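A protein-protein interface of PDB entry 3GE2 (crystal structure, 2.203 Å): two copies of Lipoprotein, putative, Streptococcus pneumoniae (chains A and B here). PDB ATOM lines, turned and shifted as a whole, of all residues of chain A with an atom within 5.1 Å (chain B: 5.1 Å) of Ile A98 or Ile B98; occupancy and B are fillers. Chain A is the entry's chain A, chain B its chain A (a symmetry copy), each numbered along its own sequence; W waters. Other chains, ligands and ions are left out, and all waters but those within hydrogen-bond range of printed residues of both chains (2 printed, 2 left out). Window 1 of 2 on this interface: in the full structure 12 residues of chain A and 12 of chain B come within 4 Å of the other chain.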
ATOM      1  N   GLN A  87      22.959  -0.321  29.421  1.00  0.00           N
ATOM      2  CA  GLN A  87      22.374   0.506  28.382  1.00  0.00           C
ATOM      3  C   GLN A  87      21.115  -0.153  27.832  1.00  0.00           C
ATOM      4  O   GLN A  87      21.079  -1.363  27.620  1.00  0.00           O
ATOM      5  CB  GLN A  87      23.411   0.716  27.253  1.00  0.00           C
ATOM      6  CG  GLN A  87      24.743   1.361  27.818  1.00  0.00           C
ATOM      7  CD  GLN A  87      24.476   2.720  28.467  1.00  0.00           C
ATOM      8  OE1 GLN A  87      23.917   3.610  27.814  1.00  0.00           O
ATOM      9  NE2 GLN A  87      24.826   2.878  29.774  1.00  0.00           N
ATOM     10  N   VAL A  88      20.087   0.654  27.602  1.00  0.00           N
ATOM     11  CA  VAL A  88      18.793   0.159  27.126  1.00  0.00           C
ATOM     12  C   VAL A  88      18.447   0.788  25.809  1.00  0.00           C
ATOM     13  O   VAL A  88      18.724   1.960  25.613  1.00  0.00           O
ATOM     14  CB  VAL A  88      17.677   0.610  28.012  1.00  0.00           C
ATOM     15  CG1 VAL A  88      16.710  -0.426  28.114  1.00  0.00           C
ATOM     16  CG2 VAL A  88      18.198   0.850  29.375  1.00  0.00           C
ATOM     17  N   THR A  89      17.792   0.027  24.934  1.00  0.00           N
ATOM     18  CA  THR A  89      17.263   0.611  23.711  1.00  0.00           C
ATOM     19  C   THR A  89      15.874   0.057  23.575  1.00  0.00           C
ATOM     20  O   THR A  89      15.623  -1.141  23.891  1.00  0.00           O
ATOM     21  CB  THR A  89      18.034   0.253  22.414  1.00  0.00           C
ATOM     22  OG1 THR A  89      18.201  -1.162  22.359  1.00  0.00           O
ATOM     23  CG2 THR A  89      19.439   0.895  22.403  1.00  0.00           C
ATOM     24  N   ARG A  96      10.245  -4.420  21.539  1.00  0.00           N
ATOM     25  CA  ARG A  96      11.443  -5.010  22.141  1.00  0.00           C
ATOM     26  C   ARG A  96      12.321  -4.011  22.887  1.00  0.00           C
ATOM     27  O   ARG A  96      12.693  -2.953  22.364  1.00  0.00           O
ATOM     28  CB  ARG A  96      12.351  -5.672  21.073  1.00  0.00           C
ATOM     29  CG  ARG A  96      11.645  -6.751  20.209  1.00  0.00           C
ATOM     30  CD  ARG A  96      11.444  -8.022  20.954  1.00  0.00           C
ATOM     31  NE  ARG A  96      11.083  -9.129  20.081  1.00  0.00           N
ATOM     32  CZ  ARG A  96       9.821  -9.541  19.878  1.00  0.00           C
ATOM     33  NH1 ARG A  96       8.791  -8.922  20.453  1.00  0.00           N
ATOM     34  NH2 ARG A  96       9.577 -10.582  19.100  1.00  0.00           N
ATOM     35  N   MET A  97      12.752  -4.404  24.068  1.00  0.00           N
ATOM     36  CA  MET A  97      13.705  -3.612  24.801  1.00  0.00           C
ATOM     37  C   MET A  97      14.933  -4.469  25.017  1.00  0.00           C
ATOM     38  O   MET A  97      14.863  -5.615  25.464  1.00  0.00           O
ATOM     39  CB  MET A  97      13.152  -3.163  26.167  1.00  0.00           C
ATOM     40  CG  MET A  97      14.193  -2.408  27.027  1.00  0.00           C
ATOM     41  SD  MET A  97      13.415  -2.193  28.911  1.00  0.00           S
ATOM     42  CE  MET A  97      13.655  -4.039  29.485  1.00  0.00           C
ATOM     43  N   ILE A  98      16.073  -3.873  24.740  1.00  0.00           N
ATOM     44  CA  ILE A  98      17.303  -4.576  24.895  1.00  0.00           C
ATOM     45  C   ILE A  98      17.986  -3.911  26.075  1.00  0.00           C
ATOM     46  O   ILE A  98      18.167  -2.682  26.109  1.00  0.00           O
ATOM     47  CB  ILE A  98      18.154  -4.366  23.641  1.00  0.00           C
ATOM     48  CG1 ILE A  98      17.475  -5.027  22.407  1.00  0.00           C
ATOM     49  CG2 ILE A  98      19.561  -4.911  23.840  1.00  0.00           C
ATOM     50  CD1 ILE A  98      18.255  -4.743  21.074  1.00  0.00           C
ATOM     51  N   ILE A  99      18.347  -4.716  27.056  1.00  0.00           N
ATOM     52  CA  ILE A  99      19.202  -4.185  28.099  1.00  0.00           C
ATOM     53  C   ILE A  99      20.513  -4.903  28.132  1.00  0.00           C
ATOM     54  O   ILE A  99      20.553  -6.110  28.313  1.00  0.00           O
ATOM     55  CB  ILE A  99      18.541  -4.270  29.445  1.00  0.00           C
ATOM     56  CG1 ILE A  99      17.926  -5.599  29.607  1.00  0.00           C
ATOM     57  CG2 ILE A  99      17.401  -3.277  29.490  1.00  0.00           C
ATOM     58  CD1 ILE A  99      16.728  -5.536  30.551  1.00  0.00           C
ATOM     59  N   GLY A 100      21.585  -4.142  27.960  1.00  0.00           N
ATOM     60  CA  GLY A 100      22.889  -4.727  27.720  1.00  0.00           C
ATOM     61  C   GLY A 100      22.787  -5.467  26.407  1.00  0.00           C
ATOM     62  O   GLY A 100      22.647  -4.855  25.351  1.00  0.00           O
ATOM     63  N   ASP A 101      22.834  -6.783  26.456  1.00  0.00           N
ATOM     64  CA  ASP A 101      22.532  -7.519  25.246  1.00  0.00           C
ATOM     65  C   ASP A 101      21.475  -8.566  25.485  1.00  0.00           C
ATOM     66  O   ASP A 101      21.419  -9.530  24.772  1.00  0.00           O
ATOM     67  CB  ASP A 101      23.777  -8.119  24.613  1.00  0.00           C
ATOM     68  CG  ASP A 101      24.363  -9.185  25.449  1.00  0.00           C
ATOM     69  OD1 ASP A 101      25.278  -9.895  24.970  1.00  0.00           O
ATOM     70  OD2 ASP A 101      23.885  -9.325  26.591  1.00  0.00           O
ATOM     71  N   ASP A 102      20.639  -8.365  26.496  1.00  0.00           N
ATOM     72  CA  ASP A 102      19.542  -9.285  26.751  1.00  0.00           C
ATOM     73  C   ASP A 102      18.248  -8.684  26.193  1.00  0.00           C
ATOM     74  O   ASP A 102      17.902  -7.541  26.482  1.00  0.00           O
ATOM     75  CB  ASP A 102      19.408  -9.540  28.252  1.00  0.00           C
ATOM     76  CG  ASP A 102      20.626 -10.269  28.836  1.00  0.00           C
ATOM     77  OD1 ASP A 102      21.252 -11.076  28.108  1.00  0.00           O
ATOM     78  OD2 ASP A 102      20.959 -10.045  30.023  1.00  0.00           O
ATOM     79  N   VAL A 103      17.532  -9.462  25.401  1.00  0.00           N
ATOM     80  CA  VAL A 103      16.299  -9.009  24.772  1.00  0.00           C
ATOM     81  C   VAL A 103      15.064  -9.235  25.633  1.00  0.00           C
ATOM     82  O   VAL A 103      14.810 -10.349  26.065  1.00  0.00           O
ATOM     83  CB  VAL A 103      16.096  -9.766  23.465  1.00  0.00           C
ATOM     84  CG1 VAL A 103      14.737  -9.364  22.777  1.00  0.00           C
ATOM     85  CG2 VAL A 103      17.289  -9.490  22.575  1.00  0.00           C
ATOM     86  N   LYS A 104      14.295  -8.173  25.877  1.00  0.00           N
ATOM     87  CA  LYS A 104      13.006  -8.269  26.570  1.00  0.00           C
ATOM     88  C   LYS A 104      11.876  -7.756  25.688  1.00  0.00           C
ATOM     89  O   LYS A 104      12.086  -7.037  24.709  1.00  0.00           O
ATOM     90  CB  LYS A 104      13.021  -7.386  27.830  1.00  0.00           C
ATOM     91  CG  LYS A 104      14.245  -7.567  28.762  1.00  0.00           C
ATOM     92  CD  LYS A 104      14.136  -8.988  29.339  1.00  0.00           C
ATOM     93  CE  LYS A 104      15.184  -9.273  30.427  1.00  0.00           C
ATOM     94  NZ  LYS A 104      14.962 -10.652  30.972  1.00  0.00           N
ATOM     95  N   GLN B  87      13.816 -15.681  13.622  1.00  0.00           N
ATOM     96  CA  GLN B  87      13.000 -14.486  13.507  1.00  0.00           C
ATOM     97  C   GLN B  87      13.855 -13.245  13.723  1.00  0.00           C
ATOM     98  O   GLN B  87      14.708 -13.212  14.608  1.00  0.00           O
ATOM     99  CB  GLN B  87      11.860 -14.546  14.550  1.00  0.00           C
ATOM    100  CG  GLN B  87      10.988 -15.856  14.364  1.00  0.00           C
ATOM    101  CD  GLN B  87      10.354 -15.916  12.974  1.00  0.00           C
ATOM    102  OE1 GLN B  87       9.647 -14.979  12.583  1.00  0.00           O
ATOM    103  NE2 GLN B  87      10.642 -16.994  12.192  1.00  0.00           N
ATOM    104  N   VAL B  88      13.616 -12.223  12.909  1.00  0.00           N
ATOM    105  CA  VAL B  88      14.393 -10.983  12.959  1.00  0.00           C
ATOM    106  C   VAL B  88      13.496  -9.816  13.251  1.00  0.00           C
ATOM    107  O   VAL B  88      12.381  -9.779  12.757  1.00  0.00           O
ATOM    108  CB  VAL B  88      14.958 -10.638  11.619  1.00  0.00           C
ATOM    109  CG1 VAL B  88      16.250 -10.072  11.785  1.00  0.00           C
ATOM    110  CG2 VAL B  88      15.127 -11.874  10.825  1.00  0.00           C
ATOM    111  N   THR B  89      14.002  -8.842  14.004  1.00  0.00           N
ATOM    112  CA  THR B  89      13.267  -7.600  14.185  1.00  0.00           C
ATOM    113  C   THR B  89      14.283  -6.509  14.013  1.00  0.00           C
ATOM    114  O   THR B  89      15.458  -6.644  14.458  1.00  0.00           O
ATOM    115  CB  THR B  89      12.612  -7.410  15.577  1.00  0.00           C
ATOM    116  OG1 THR B  89      13.595  -7.656  16.580  1.00  0.00           O
ATOM    117  CG2 THR B  89      11.456  -8.412  15.794  1.00  0.00           C
ATOM    118  N   ARG B  96      19.461  -1.382  15.678  1.00  0.00           N
ATOM    119  CA  ARG B  96      19.617  -2.745  16.191  1.00  0.00           C
ATOM    120  C   ARG B  96      18.766  -3.783  15.468  1.00  0.00           C
ATOM    121  O   ARG B  96      17.551  -3.624  15.295  1.00  0.00           O
ATOM    122  CB  ARG B  96      19.232  -2.836  17.691  1.00  0.00           C
ATOM    123  CG  ARG B  96      20.011  -1.863  18.615  1.00  0.00           C
ATOM    124  CD  ARG B  96      21.406  -2.318  18.854  1.00  0.00           C
ATOM    125  NE  ARG B  96      22.042  -1.607  19.954  1.00  0.00           N
ATOM    126  CZ  ARG B  96      22.860  -0.554  19.791  1.00  0.00           C
ATOM    127  NH1 ARG B  96      23.121  -0.061  18.581  1.00  0.00           N
ATOM    128  NH2 ARG B  96      23.433   0.014  20.840  1.00  0.00           N
ATOM    129  N   MET B  97      19.383  -4.902  15.150  1.00  0.00           N
ATOM    130  CA  MET B  97      18.650  -6.012  14.599  1.00  0.00           C
ATOM    131  C   MET B  97      18.827  -7.182  15.541  1.00  0.00           C
ATOM    132  O   MET B  97      19.935  -7.534  15.950  1.00  0.00           O
ATOM    133  CB  MET B  97      19.164  -6.404  13.201  1.00  0.00           C
ATOM    134  CG  MET B  97      18.473  -7.666  12.630  1.00  0.00           C
ATOM    135  SD  MET B  97      19.499  -8.237  10.950  1.00  0.00           S
ATOM    136  CE  MET B  97      21.054  -8.981  11.856  1.00  0.00           C
ATOM    137  N   ILE B  98      17.715  -7.818  15.842  1.00  0.00           N
ATOM    138  CA  ILE B  98      17.746  -8.935  16.725  1.00  0.00           C
ATOM    139  C   ILE B  98      17.433 -10.135  15.851  1.00  0.00           C
ATOM    140  O   ILE B  98      16.420 -10.163  15.131  1.00  0.00           O
ATOM    141  CB  ILE B  98      16.637  -8.773  17.767  1.00  0.00           C
ATOM    142  CG1 ILE B  98      16.921  -7.542  18.676  1.00  0.00           C
ATOM    143  CG2 ILE B  98      16.483 -10.036  18.601  1.00  0.00           C
ATOM    144  CD1 ILE B  98      15.754  -7.267  19.689  1.00  0.00           C
ATOM    145  N   ILE B  99      18.311 -11.118  15.891  1.00  0.00           N
ATOM    146  CA  ILE B  99      17.961 -12.377  15.264  1.00  0.00           C
ATOM    147  C   ILE B  99      17.912 -13.480  16.272  1.00  0.00           C
ATOM    148  O   ILE B  99      18.899 -13.755  16.937  1.00  0.00           O
ATOM    149  CB  ILE B  99      18.925 -12.729  14.168  1.00  0.00           C
ATOM    150  CG1 ILE B  99      20.305 -12.502  14.636  1.00  0.00           C
ATOM    151  CG2 ILE B  99      18.717 -11.777  13.012  1.00  0.00           C
ATOM    152  CD1 ILE B  99      21.230 -12.174  13.468  1.00  0.00           C
ATOM    153  N   GLY B 100      16.751 -14.112  16.370  1.00  0.00           N
ATOM    154  CA  GLY B 100      16.484 -15.023  17.465  1.00  0.00           C
ATOM    155  C   GLY B 100      16.524 -14.194  18.727  1.00  0.00           C
ATOM    156  O   GLY B 100      15.657 -13.354  18.953  1.00  0.00           O
ATOM    157  N   ASP B 101      17.533 -14.402  19.548  1.00  0.00           N
ATOM    158  CA  ASP B 101      17.709 -13.485  20.654  1.00  0.00           C
ATOM    159  C   ASP B 101      19.111 -12.936  20.700  1.00  0.00           C
ATOM    160  O   ASP B 101      19.565 -12.546  21.741  1.00  0.00           O
ATOM    161  CB  ASP B 101      17.309 -14.103  21.984  1.00  0.00           C
ATOM    162  CG  ASP B 101      18.218 -15.195  22.381  1.00  0.00           C
ATOM    163  OD1 ASP B 101      18.125 -15.670  23.536  1.00  0.00           O
ATOM    164  OD2 ASP B 101      19.050 -15.566  21.530  1.00  0.00           O
ATOM    165  N   ASP B 102      19.792 -12.913  19.561  1.00  0.00           N
ATOM    166  CA  ASP B 102      21.124 -12.331  19.499  1.00  0.00           C
ATOM    167  C   ASP B 102      21.024 -10.922  18.909  1.00  0.00           C
ATOM    168  O   ASP B 102      20.436 -10.716  17.849  1.00  0.00           O
ATOM    169  CB  ASP B 102      22.040 -13.205  18.643  1.00  0.00           C
ATOM    170  CG  ASP B 102      22.285 -14.586  19.265  1.00  0.00           C
ATOM    171  OD1 ASP B 102      22.292 -14.693  20.515  1.00  0.00           O
ATOM    172  OD2 ASP B 102      22.478 -15.569  18.510  1.00  0.00           O
ATOM    173  N   VAL B 103      21.610  -9.955  19.593  1.00  0.00           N
ATOM    174  CA  VAL B 103      21.563  -8.562  19.168  1.00  0.00           C
ATOM    175  C   VAL B 103      22.692  -8.183  18.219  1.00  0.00           C
ATOM    176  O   VAL B 103      23.855  -8.381  18.537  1.00  0.00           O
ATOM    177  CB  VAL B 103      21.666  -7.661  20.393  1.00  0.00           C
ATOM    178  CG1 VAL B 103      21.693  -6.141  19.982  1.00  0.00           C
ATOM    179  CG2 VAL B 103      20.505  -7.984  21.308  1.00  0.00           C
ATOM    180  N   LYS B 104      22.345  -7.634  17.055  1.00  0.00           N
ATOM    181  CA  LYS B 104      23.326  -7.094  16.108  1.00  0.00           C
ATOM    182  C   LYS B 104      23.074  -5.614  15.852  1.00  0.00           C
ATOM    183  O   LYS B 104      21.995  -5.079  16.114  1.00  0.00           O
ATOM    184  CB  LYS B 104      23.193  -7.807  14.752  1.00  0.00           C
ATOM    185  CG  LYS B 104      23.168  -9.354  14.807  1.00  0.00           C
ATOM    186  CD  LYS B 104      24.562  -9.789  15.289  1.00  0.00           C
ATOM    187  CE  LYS B 104      24.767 -11.311  15.234  1.00  0.00           C
ATOM    188  NZ  LYS B 104      26.166 -11.633  15.660  1.00  0.00           N
HETATM  189  O   HOH W   1      20.930  -2.277  22.373  1.00  0.00           O
HETATM  190  O   HOH W   2      13.178  -9.876  18.472  1.00  0.00           O
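Ile B98 touches Ile A98.
Ile A98 touches Val B103.
O of Asp A101 touches CG2 of Val B103, at 3.9 Å.
Val A103 touches Ile B98.
CG2 of Val A103 touches O of Asp B101 (3.9 Å).
CG2 of Val B103 touches CG2 of Val A103, at 3.8 Å.
O of Thr A89 is in hydrogen-bond range of N of Ile A98 (2.9 Å).
O of Thr B89 lies within hydrogen-bond range of N of Ile B98, 2.9 Å away.
Printed residues of chain A that touch a printed residue of chain B: Ile A98, Asp A101 and Val A103.
Hydrophobic or aromatic side chains of chain B within 4 Å of the printed part of chain A: Ile B98 and Val B103.
Among the printed residues, 6 pairs touch across the chains.
Among the printed residues, no Asp or Glu carboxylate lies within 4 Å of a Lys or Arg side-chain nitrogen of the other chain.
Ile B98 touches its own counterpart, Ile A98.
Ile A98 touches Val B103, and with the chains exchanged Val A103 touches Ile B98.
Asp A101 touches Val B103, and with the chains exchanged Val A103 touches Asp B101.
Val A103 touches its own counterpart, Val B103.
12 positions are printed for both chains.
Of the 6 pairs that touch across the chains among the printed residues, 6 have their exchanged pair printed and touching as well.
Printed residues of chain B within 4 Å of Ile A98: Ile B98 and Val B103.
Printed residues of chain B within 4 Å of Asp A101: Val B103 (3.9 Å).
Of the printed residues of chain B, Val A103 touches Ile B98 (3.9 Å), Asp B101 (3.9 Å) and Val B103 (3.8 Å).
Of the printed residues of chain A, Ile B98 touches Ile A98 and Val A103.
Ile B99 touches none of the printed residues of chain A.
Printed residues of chain A within 4 Å of Asp B101: Val A103 (3.9 Å).
Water W2 lies within hydrogen-bond range of NE of Arg A96 (2.7 Å) and OG1 of Thr B89 (2.9 Å).
Water W1 bridges the guanidinium group of Arg B96 (2.7 Å) and the side-chain hydroxyl of Thr A89 (2.9 Å).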
